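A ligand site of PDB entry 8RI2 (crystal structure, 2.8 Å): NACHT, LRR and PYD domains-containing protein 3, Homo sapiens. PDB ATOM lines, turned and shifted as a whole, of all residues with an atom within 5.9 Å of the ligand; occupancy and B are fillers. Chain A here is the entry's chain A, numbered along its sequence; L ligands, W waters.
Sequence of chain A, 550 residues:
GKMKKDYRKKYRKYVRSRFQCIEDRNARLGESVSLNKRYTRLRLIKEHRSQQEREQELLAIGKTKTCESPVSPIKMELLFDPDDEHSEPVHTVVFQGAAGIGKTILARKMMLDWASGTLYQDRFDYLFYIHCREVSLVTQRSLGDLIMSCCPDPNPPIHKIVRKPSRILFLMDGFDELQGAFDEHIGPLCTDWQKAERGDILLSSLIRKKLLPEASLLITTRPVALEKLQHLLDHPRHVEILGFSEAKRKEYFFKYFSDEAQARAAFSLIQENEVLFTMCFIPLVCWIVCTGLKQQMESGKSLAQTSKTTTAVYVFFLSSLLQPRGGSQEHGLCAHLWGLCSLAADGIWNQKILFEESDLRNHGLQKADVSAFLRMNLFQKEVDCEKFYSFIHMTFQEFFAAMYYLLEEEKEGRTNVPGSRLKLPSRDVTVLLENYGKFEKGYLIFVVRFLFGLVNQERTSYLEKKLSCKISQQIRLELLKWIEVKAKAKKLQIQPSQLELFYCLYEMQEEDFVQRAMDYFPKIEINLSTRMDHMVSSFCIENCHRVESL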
ATOM      1  N   ILE A  22       9.268  25.571  31.559  1.00  0.00           N
ATOM      2  CA  ILE A  22       9.544  25.119  30.193  1.00  0.00           C
ATOM      3  C   ILE A  22      10.216  23.734  30.120  1.00  0.00           C
ATOM      4  O   ILE A  22       9.834  22.901  29.286  1.00  0.00           O
ATOM      5  CB  ILE A  22      10.390  26.217  29.506  1.00  0.00           C
ATOM      6  CG1 ILE A  22       9.583  27.521  29.342  1.00  0.00           C
ATOM      7  CG2 ILE A  22      10.984  25.750  28.183  1.00  0.00           C
ATOM      8  CD1 ILE A  22      10.373  28.719  28.828  1.00  0.00           C
ATOM      9  N   ARG A  38       8.710  33.432  30.722  1.00  0.00           N
ATOM     10  CA  ARG A  38       9.265  33.579  29.376  1.00  0.00           C
ATOM     11  C   ARG A  38       8.236  33.169  28.303  1.00  0.00           C
ATOM     12  O   ARG A  38       8.472  33.449  27.127  1.00  0.00           O
ATOM     13  CB  ARG A  38      10.550  32.746  29.225  1.00  0.00           C
ATOM     14  CG  ARG A  38      11.671  33.449  28.461  1.00  0.00           C
ATOM     15  CD  ARG A  38      12.565  32.448  27.774  1.00  0.00           C
ATOM     16  NE  ARG A  38      13.864  32.277  28.440  1.00  0.00           N
ATOM     17  CZ  ARG A  38      14.663  31.223  28.264  1.00  0.00           C
ATOM     18  NH1 ARG A  38      14.291  30.226  27.472  1.00  0.00           N
ATOM     19  NH2 ARG A  38      15.829  31.155  28.887  1.00  0.00           N
ATOM     20  N   TYR A  39       7.102  32.531  28.689  1.00  0.00           N
ATOM     21  CA  TYR A  39       6.037  32.146  27.749  1.00  0.00           C
ATOM     22  C   TYR A  39       5.471  33.411  27.111  1.00  0.00           C
ATOM     23  O   TYR A  39       4.983  34.304  27.811  1.00  0.00           O
ATOM     24  CB  TYR A  39       4.899  31.339  28.435  1.00  0.00           C
ATOM     25  CG  TYR A  39       3.773  31.014  27.481  1.00  0.00           C
ATOM     26  CD1 TYR A  39       3.828  29.907  26.655  1.00  0.00           C
ATOM     27  CD2 TYR A  39       2.692  31.878  27.321  1.00  0.00           C
ATOM     28  CE1 TYR A  39       2.838  29.638  25.725  1.00  0.00           C
ATOM     29  CE2 TYR A  39       1.712  31.643  26.368  1.00  0.00           C
ATOM     30  CZ  TYR A  39       1.788  30.517  25.575  1.00  0.00           C
ATOM     31  OH  TYR A  39       0.805  30.271  24.629  1.00  0.00           O
ATOM     32  N   THR A  40       5.538  33.472  25.777  1.00  0.00           N
ATOM     33  CA  THR A  40       5.007  34.584  24.981  1.00  0.00           C
ATOM     34  C   THR A  40       3.787  34.064  24.207  1.00  0.00           C
ATOM     35  O   THR A  40       3.835  32.932  23.731  1.00  0.00           O
ATOM     36  CB  THR A  40       6.146  35.157  24.102  1.00  0.00           C
ATOM     37  OG1 THR A  40       7.181  35.645  24.951  1.00  0.00           O
ATOM     38  CG2 THR A  40       5.673  36.252  23.170  1.00  0.00           C
ATOM     39  N   ARG A  41       2.696  34.846  24.091  1.00  0.00           N
ATOM     40  CA  ARG A  41       1.499  34.380  23.385  1.00  0.00           C
ATOM     41  C   ARG A  41       1.772  33.844  21.982  1.00  0.00           C
ATOM     42  O   ARG A  41       2.662  34.332  21.298  1.00  0.00           O
ATOM     43  CB  ARG A  41       0.386  35.454  23.354  1.00  0.00           C
ATOM     44  CG  ARG A  41      -1.046  34.893  23.495  1.00  0.00           C
ATOM     45  CD  ARG A  41      -2.140  35.830  22.958  1.00  0.00           C
ATOM     46  NE  ARG A  41      -2.094  35.911  21.497  1.00  0.00           N
ATOM     47  CZ  ARG A  41      -2.109  37.049  20.810  1.00  0.00           C
ATOM     48  NH1 ARG A  41      -2.024  37.025  19.484  1.00  0.00           N
ATOM     49  NH2 ARG A  41      -2.198  38.212  21.440  1.00  0.00           N
ATOM     50  N   LEU A  42       1.069  32.786  21.591  1.00  0.00           N
ATOM     51  CA  LEU A  42       1.225  32.199  20.275  1.00  0.00           C
ATOM     52  C   LEU A  42       0.021  32.521  19.400  1.00  0.00           C
ATOM     53  O   LEU A  42      -1.102  32.637  19.898  1.00  0.00           O
ATOM     54  CB  LEU A  42       1.451  30.680  20.372  1.00  0.00           C
ATOM     55  CG  LEU A  42       2.850  30.237  20.745  1.00  0.00           C
ATOM     56  CD1 LEU A  42       2.921  28.765  20.970  1.00  0.00           C
ATOM     57  CD2 LEU A  42       3.851  30.635  19.682  1.00  0.00           C
ATOM     58  N   GLY A  97       1.251  22.370  13.948  1.00  0.00           N
ATOM     59  CA  GLY A  97       2.332  23.318  14.093  1.00  0.00           C
ATOM     60  C   GLY A  97       3.644  22.736  13.632  1.00  0.00           C
ATOM     61  O   GLY A  97       3.936  21.570  13.878  1.00  0.00           O
ATOM     62  N   ALA A  98       4.460  23.538  12.952  1.00  0.00           N
ATOM     63  CA  ALA A  98       5.740  23.094  12.437  1.00  0.00           C
ATOM     64  C   ALA A  98       6.803  22.903  13.566  1.00  0.00           C
ATOM     65  O   ALA A  98       6.548  23.300  14.705  1.00  0.00           O
ATOM     66  CB  ALA A  98       6.227  24.058  11.374  1.00  0.00           C
ATOM     67  N   ALA A  99       7.962  22.260  13.255  1.00  0.00           N
ATOM     68  CA  ALA A  99       9.044  22.030  14.223  1.00  0.00           C
ATOM     69  C   ALA A  99       9.443  23.323  14.923  1.00  0.00           C
ATOM     70  O   ALA A  99       9.549  24.341  14.272  1.00  0.00           O
ATOM     71  CB  ALA A  99      10.233  21.423  13.507  1.00  0.00           C
ATOM     72  N   GLY A 100       9.541  23.305  16.231  1.00  0.00           N
ATOM     73  CA  GLY A 100       9.918  24.480  17.007  1.00  0.00           C
ATOM     74  C   GLY A 100       8.906  25.608  17.115  1.00  0.00           C
ATOM     75  O   GLY A 100       9.226  26.646  17.693  1.00  0.00           O
ATOM     76  N   ILE A 101       7.676  25.432  16.596  1.00  0.00           N
ATOM     77  CA  ILE A 101       6.664  26.505  16.672  1.00  0.00           C
ATOM     78  C   ILE A 101       6.062  26.674  18.091  1.00  0.00           C
ATOM     79  O   ILE A 101       5.420  27.690  18.381  1.00  0.00           O
ATOM     80  CB  ILE A 101       5.554  26.321  15.583  1.00  0.00           C
ATOM     81  CG1 ILE A 101       5.032  27.657  15.075  1.00  0.00           C
ATOM     82  CG2 ILE A 101       4.407  25.435  16.073  1.00  0.00           C
ATOM     83  CD1 ILE A 101       5.985  28.425  14.263  1.00  0.00           C
ATOM     84  N   GLY A 102       6.232  25.689  18.962  1.00  0.00           N
ATOM     85  CA  GLY A 102       5.713  25.752  20.316  1.00  0.00           C
ATOM     86  C   GLY A 102       4.580  24.796  20.649  1.00  0.00           C
ATOM     87  O   GLY A 102       3.728  25.139  21.466  1.00  0.00           O
ATOM     88  N   LYS A 103       4.554  23.595  20.047  1.00  0.00           N
ATOM     89  CA  LYS A 103       3.506  22.626  20.314  1.00  0.00           C
ATOM     90  C   LYS A 103       3.584  22.145  21.777  1.00  0.00           C
ATOM     91  O   LYS A 103       2.575  22.134  22.485  1.00  0.00           O
ATOM     92  CB  LYS A 103       3.596  21.421  19.361  1.00  0.00           C
ATOM     93  CG  LYS A 103       3.214  21.711  17.903  1.00  0.00           C
ATOM     94  CD  LYS A 103       3.781  20.645  16.977  1.00  0.00           C
ATOM     95  CE  LYS A 103       5.280  20.777  16.892  1.00  0.00           C
ATOM     96  NZ  LYS A 103       5.884  19.752  16.005  1.00  0.00           N
ATOM     97  N   THR A 104       4.800  21.745  22.209  1.00  0.00           N
ATOM     98  CA  THR A 104       5.048  21.274  23.557  1.00  0.00           C
ATOM     99  C   THR A 104       4.873  22.392  24.566  1.00  0.00           C
ATOM    100  O   THR A 104       4.305  22.181  25.645  1.00  0.00           O
ATOM    101  CB  THR A 104       6.455  20.667  23.648  1.00  0.00           C
ATOM    102  OG1 THR A 104       6.526  19.508  22.816  1.00  0.00           O
ATOM    103  CG2 THR A 104       6.832  20.291  25.078  1.00  0.00           C
ATOM    104  N   ILE A 105       5.351  23.600  24.220  1.00  0.00           N
ATOM    105  CA  ILE A 105       5.229  24.725  25.128  1.00  0.00           C
ATOM    106  C   ILE A 105       3.776  25.112  25.360  1.00  0.00           C
ATOM    107  O   ILE A 105       3.395  25.399  26.488  1.00  0.00           O
ATOM    108  CB  ILE A 105       6.125  25.881  24.674  1.00  0.00           C
ATOM    109  CG1 ILE A 105       7.588  25.420  24.640  1.00  0.00           C
ATOM    110  CG2 ILE A 105       5.937  27.098  25.563  1.00  0.00           C
ATOM    111  CD1 ILE A 105       8.125  24.937  25.982  1.00  0.00           C
ATOM    112  N   LEU A 106       2.934  25.009  24.320  1.00  0.00           N
ATOM    113  CA  LEU A 106       1.512  25.303  24.445  1.00  0.00           C
ATOM    114  C   LEU A 106       0.777  24.230  25.259  1.00  0.00           C
ATOM    115  O   LEU A 106      -0.130  24.556  26.028  1.00  0.00           O
ATOM    116  CB  LEU A 106       0.878  25.443  23.064  1.00  0.00           C
ATOM    117  CG  LEU A 106      -0.539  25.997  23.033  1.00  0.00           C
ATOM    118  CD1 LEU A 106      -0.637  27.333  23.769  1.00  0.00           C
ATOM    119  CD2 LEU A 106      -0.995  26.180  21.619  1.00  0.00           C
ATOM    120  N   ASP A 173       0.726  15.055  22.952  1.00  0.00           N
ATOM    121  CA  ASP A 173       1.692  16.004  22.431  1.00  0.00           C
ATOM    122  C   ASP A 173       2.709  15.367  21.490  1.00  0.00           C
ATOM    123  O   ASP A 173       3.414  14.435  21.871  1.00  0.00           O
ATOM    124  CB  ASP A 173       2.370  16.766  23.574  1.00  0.00           C
ATOM    125  CG  ASP A 173       3.445  17.757  23.150  1.00  0.00           C
ATOM    126  OD1 ASP A 173       3.332  18.317  22.041  1.00  0.00           O
ATOM    127  OD2 ASP A 173       4.394  17.967  23.944  1.00  0.00           O
ATOM    128  N   GLU A 177       5.987  12.461  16.616  1.00  0.00           N
ATOM    129  CA  GLU A 177       7.111  11.911  17.342  1.00  0.00           C
ATOM    130  C   GLU A 177       6.870  10.485  17.847  1.00  0.00           C
ATOM    131  O   GLU A 177       7.592  10.027  18.726  1.00  0.00           O
ATOM    132  CB  GLU A 177       7.491  12.814  18.514  1.00  0.00           C
ATOM    133  CG  GLU A 177       7.865  14.220  18.099  1.00  0.00           C
ATOM    134  CD  GLU A 177       8.630  14.971  19.166  1.00  0.00           C
ATOM    135  OE1 GLU A 177       8.273  14.840  20.364  1.00  0.00           O
ATOM    136  OE2 GLU A 177       9.584  15.700  18.808  1.00  0.00           O
ATOM    137  N   PHE A 244       5.086  33.373  16.387  1.00  0.00           N
ATOM    138  CA  PHE A 244       5.131  34.717  16.939  1.00  0.00           C
ATOM    139  C   PHE A 244       4.778  35.810  15.973  1.00  0.00           C
ATOM    140  O   PHE A 244       5.298  35.856  14.870  1.00  0.00           O
ATOM    141  CB  PHE A 244       6.534  35.005  17.491  1.00  0.00           C
ATOM    142  CG  PHE A 244       6.889  34.357  18.809  1.00  0.00           C
ATOM    143  CD1 PHE A 244       5.897  33.986  19.701  1.00  0.00           C
ATOM    144  CD2 PHE A 244       8.209  34.142  19.156  1.00  0.00           C
ATOM    145  CE1 PHE A 244       6.231  33.386  20.908  1.00  0.00           C
ATOM    146  CE2 PHE A 244       8.534  33.570  20.377  1.00  0.00           C
ATOM    147  CZ  PHE A 244       7.535  33.184  21.244  1.00  0.00           C
ATOM    148  N   TYR A 252       9.411  38.463  23.074  1.00  0.00           N
ATOM    149  CA  TYR A 252      10.330  37.376  23.424  1.00  0.00           C
ATOM    150  C   TYR A 252      11.726  37.896  23.716  1.00  0.00           C
ATOM    151  O   TYR A 252      12.276  37.608  24.775  1.00  0.00           O
ATOM    152  CB  TYR A 252      10.368  36.275  22.343  1.00  0.00           C
ATOM    153  CG  TYR A 252      11.244  35.107  22.750  1.00  0.00           C
ATOM    154  CD1 TYR A 252      12.614  35.136  22.529  1.00  0.00           C
ATOM    155  CD2 TYR A 252      10.712  34.018  23.420  1.00  0.00           C
ATOM    156  CE1 TYR A 252      13.430  34.102  22.959  1.00  0.00           C
ATOM    157  CE2 TYR A 252      11.517  32.975  23.845  1.00  0.00           C
ATOM    158  CZ  TYR A 252      12.881  33.016  23.616  1.00  0.00           C
ATOM    159  OH  TYR A 252      13.670  31.998  24.031  1.00  0.00           O
ATOM    160  N   PRO A 283       9.259  30.342  17.360  1.00  0.00           N
ATOM    161  CA  PRO A 283       9.835  30.620  18.686  1.00  0.00           C
ATOM    162  C   PRO A 283      11.177  29.922  18.931  1.00  0.00           C
ATOM    163  O   PRO A 283      12.043  30.530  19.534  1.00  0.00           O
ATOM    164  CB  PRO A 283       8.744  30.159  19.651  1.00  0.00           C
ATOM    165  CG  PRO A 283       7.482  30.233  18.850  1.00  0.00           C
ATOM    166  CD  PRO A 283       7.900  29.769  17.485  1.00  0.00           C
ATOM    167  N   LEU A 284      11.385  28.692  18.421  1.00  0.00           N
ATOM    168  CA  LEU A 284      12.679  28.020  18.567  1.00  0.00           C
ATOM    169  C   LEU A 284      13.796  28.855  17.902  1.00  0.00           C
ATOM    170  O   LEU A 284      14.873  28.979  18.479  1.00  0.00           O
ATOM    171  CB  LEU A 284      12.618  26.599  17.996  1.00  0.00           C
ATOM    172  CG  LEU A 284      13.957  25.855  17.844  1.00  0.00           C
ATOM    173  CD1 LEU A 284      14.553  25.512  19.186  1.00  0.00           C
ATOM    174  CD2 LEU A 284      13.794  24.635  17.006  1.00  0.00           C
ATOM    175  N   TRP A 287      14.771  31.599  20.245  1.00  0.00           N
ATOM    176  CA  TRP A 287      15.621  31.089  21.311  1.00  0.00           C
ATOM    177  C   TRP A 287      17.052  30.859  20.844  1.00  0.00           C
ATOM    178  O   TRP A 287      18.000  31.214  21.541  1.00  0.00           O
ATOM    179  CB  TRP A 287      15.053  29.798  21.933  1.00  0.00           C
ATOM    180  CG  TRP A 287      15.921  29.230  23.024  1.00  0.00           C
ATOM    181  CD1 TRP A 287      15.924  29.590  24.332  1.00  0.00           C
ATOM    182  CD2 TRP A 287      16.959  28.243  22.877  1.00  0.00           C
ATOM    183  NE1 TRP A 287      16.891  28.887  25.022  1.00  0.00           N
ATOM    184  CE2 TRP A 287      17.537  28.050  24.150  1.00  0.00           C
ATOM    185  CE3 TRP A 287      17.444  27.495  21.796  1.00  0.00           C
ATOM    186  CZ2 TRP A 287      18.579  27.136  24.365  1.00  0.00           C
ATOM    187  CZ3 TRP A 287      18.479  26.603  22.013  1.00  0.00           C
ATOM    188  CH2 TRP A 287      19.029  26.433  23.285  1.00  0.00           C
ATOM    189  N   ILE A 392      18.583  18.932  22.391  1.00  0.00           N
ATOM    190  CA  ILE A 392      17.816  20.091  22.868  1.00  0.00           C
ATOM    191  C   ILE A 392      16.499  20.303  22.070  1.00  0.00           C
ATOM    192  O   ILE A 392      15.536  20.839  22.606  1.00  0.00           O
ATOM    193  CB  ILE A 392      18.683  21.367  22.954  1.00  0.00           C
ATOM    194  CG1 ILE A 392      18.209  22.306  24.096  1.00  0.00           C
ATOM    195  CG2 ILE A 392      18.823  22.070  21.620  1.00  0.00           C
ATOM    196  CD1 ILE A 392      17.109  23.391  23.776  1.00  0.00           C
ATOM    197  N   HIS A 393      16.439  19.779  20.830  1.00  0.00           N
ATOM    198  CA  HIS A 393      15.268  19.790  19.954  1.00  0.00           C
ATOM    199  C   HIS A 393      15.427  18.723  18.857  1.00  0.00           C
ATOM    200  O   HIS A 393      16.508  18.198  18.645  1.00  0.00           O
ATOM    201  CB  HIS A 393      14.987  21.194  19.370  1.00  0.00           C
ATOM    202  CG  HIS A 393      13.603  21.341  18.795  1.00  0.00           C
ATOM    203  ND1 HIS A 393      13.347  21.123  17.454  1.00  0.00           N
ATOM    204  CD2 HIS A 393      12.440  21.642  19.403  1.00  0.00           C
ATOM    205  CE1 HIS A 393      12.055  21.304  17.295  1.00  0.00           C
ATOM    206  NE2 HIS A 393      11.458  21.616  18.439  1.00  0.00           N
HETATM  207  P1  LIG L   1       7.555  21.918  18.987  1.00  0.00           P
HETATM  208  O1  LIG L   1       6.859  21.085  20.047  1.00  0.00           O
HETATM  209  O2  LIG L   1       8.448  21.090  18.072  1.00  0.00           O
HETATM  210  O3  LIG L   1       6.598  22.804  18.211  1.00  0.00           O
HETATM  211  P2  LIG L   1       8.471  23.385  21.365  1.00  0.00           P
HETATM  212  O4  LIG L   1       7.098  23.781  21.711  1.00  0.00           O
HETATM  213  O5  LIG L   1       9.154  22.342  22.169  1.00  0.00           O
HETATM  214  O6  LIG L   1       8.461  22.921  19.835  1.00  0.00           O
HETATM  215  O7  LIG L   1       9.355  24.721  21.362  1.00  0.00           O
HETATM  216  C1  LIG L   1      10.808  24.705  21.405  1.00  0.00           C
HETATM  217  C2  LIG L   1      11.322  25.965  22.073  1.00  0.00           C
HETATM  218  O8  LIG L   1      10.614  27.104  21.544  1.00  0.00           O
HETATM  219  C3  LIG L   1      11.101  26.051  23.588  1.00  0.00           C
HETATM  220  O9  LIG L   1      12.141  25.415  24.318  1.00  0.00           O
HETATM  221  C4  LIG L   1      11.100  27.560  23.826  1.00  0.00           C
HETATM  222  O10 LIG L   1      12.393  28.123  24.050  1.00  0.00           O
HETATM  223  C5  LIG L   1      10.455  28.090  22.541  1.00  0.00           C
HETATM  224  N1  LIG L   1       9.033  28.384  22.667  1.00  0.00           N
HETATM  225  C6  LIG L   1       7.997  27.766  22.032  1.00  0.00           C
HETATM  226  N2  LIG L   1       6.822  28.306  22.256  1.00  0.00           N
HETATM  227  C7  LIG L   1       7.120  29.371  23.096  1.00  0.00           C
HETATM  228  C8  LIG L   1       6.311  30.378  23.679  1.00  0.00           C
HETATM  229  N3  LIG L   1       5.005  30.467  23.477  1.00  0.00           N
HETATM  230  N4  LIG L   1       6.914  31.300  24.448  1.00  0.00           N
HETATM  231  C9  LIG L   1       8.237  31.224  24.625  1.00  0.00           C
HETATM  232  N5  LIG L   1       9.107  30.339  24.123  1.00  0.00           N
HETATM  233  C10 LIG L   1       8.473  29.428  23.359  1.00  0.00           C
HETATM  234  O   HOH W   1       5.890  18.252  20.170  1.00  0.00           O
HETATM  235  O   HOH W   2      14.897  25.688  24.993  1.00  0.00           O
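A ring nitrogen (NE2) of His 393 lies within hydrogen-bond range of an oxygen (O2) of the ligand, 3.1 Å away. The side-chain hydroxyl of Thr 104 lies within hydrogen-bond range of an oxygen (O1) of the ligand (3.2 Å). The backbone NH (N) of Ile 105 is in hydrogen-bond range of an oxygen (O4) of the ligand. The backbone NH (N) of Ile 101 sits at hydrogen-bond distance from an oxygen (O3) of the ligand, at 3.3 Å. NZ of Lys 103 lies within salt-bridge range of O2 of the ligand (3.6 Å). The backbone NH of Thr 40 lies within hydrogen-bond range of a nitrogen (N4) of the ligand, at 2.9 Å. N of Gly 102 is in hydrogen-bond range of O3 of the ligand (3.0 Å). The backbone carbonyl oxygen (O) of Thr 40 lies within hydrogen-bond range of a nitrogen (N3) of the ligand, at 2.7 Å. O2 of the ligand sits at hydrogen-bond distance from N of Gly 100. The backbone NH (N) of Lys 103 lies close to an oxygen (O3) of the ligand (2.9 Å). N of Thr 104 is in hydrogen-bond range of O1 of the ligand (3.1 Å).
NE2 of His 393 sits at hydrogen-bond distance from N of Gly 100 (3.4 Å). OG1 of Thr 40 is in hydrogen-bond range of O of Arg 38. NZ of Lys 103 sits close to O of Gly 97, 3.4 Å away. O of Gly 100 is in hydrogen-bond range of N of Leu 284 (3.1 Å). OD2 of Asp 173 sits at hydrogen-bond distance from OG1 of Thr 104 (2.9 Å).
Arg 38 touches the ligand (O to C9, 3.4 Å). Tyr 39 touches the ligand. Leu 42 touches the ligand. O of Ala 98 touches O3 of the ligand, 3.5 Å away. C of Ala 99 touches O2 of the ligand (3.99 Å). Phe 244 touches the ligand. CE2 of Tyr 252 touches N5 of the ligand, 3.6 Å away. Pro 283 touches the ligand (CB to C6, 3.5 Å). N of Leu 284 touches O8 of the ligand, 3.6 Å away. Trp 287 touches the ligand. Hydrophobic or aromatic side chains that line the ligand: Tyr 39, Leu 42, Ile 105, Phe 244, Tyr 252, Pro 283, Trp 287 and His 393. 18 residues have an atom within 4 Å of the ligand: Arg 38, Tyr 39, Thr 40, Leu 42, Ala 98, Ala 99, Gly 100, Ile 101, Gly 102, Lys 103, Thr 104, Ile 105, Phe 244, Tyr 252, Pro 283, Leu 284, Trp 287 and His 393. The nearest printed residue that does not touch the ligand is Ile 22 (4.05 Å).
Water W1 lies within hydrogen-bond range of O1 of the ligand (3.0 Å), OG1 of Thr 104 (3.0 Å) and OD1 of Asp 173 (3.2 Å).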
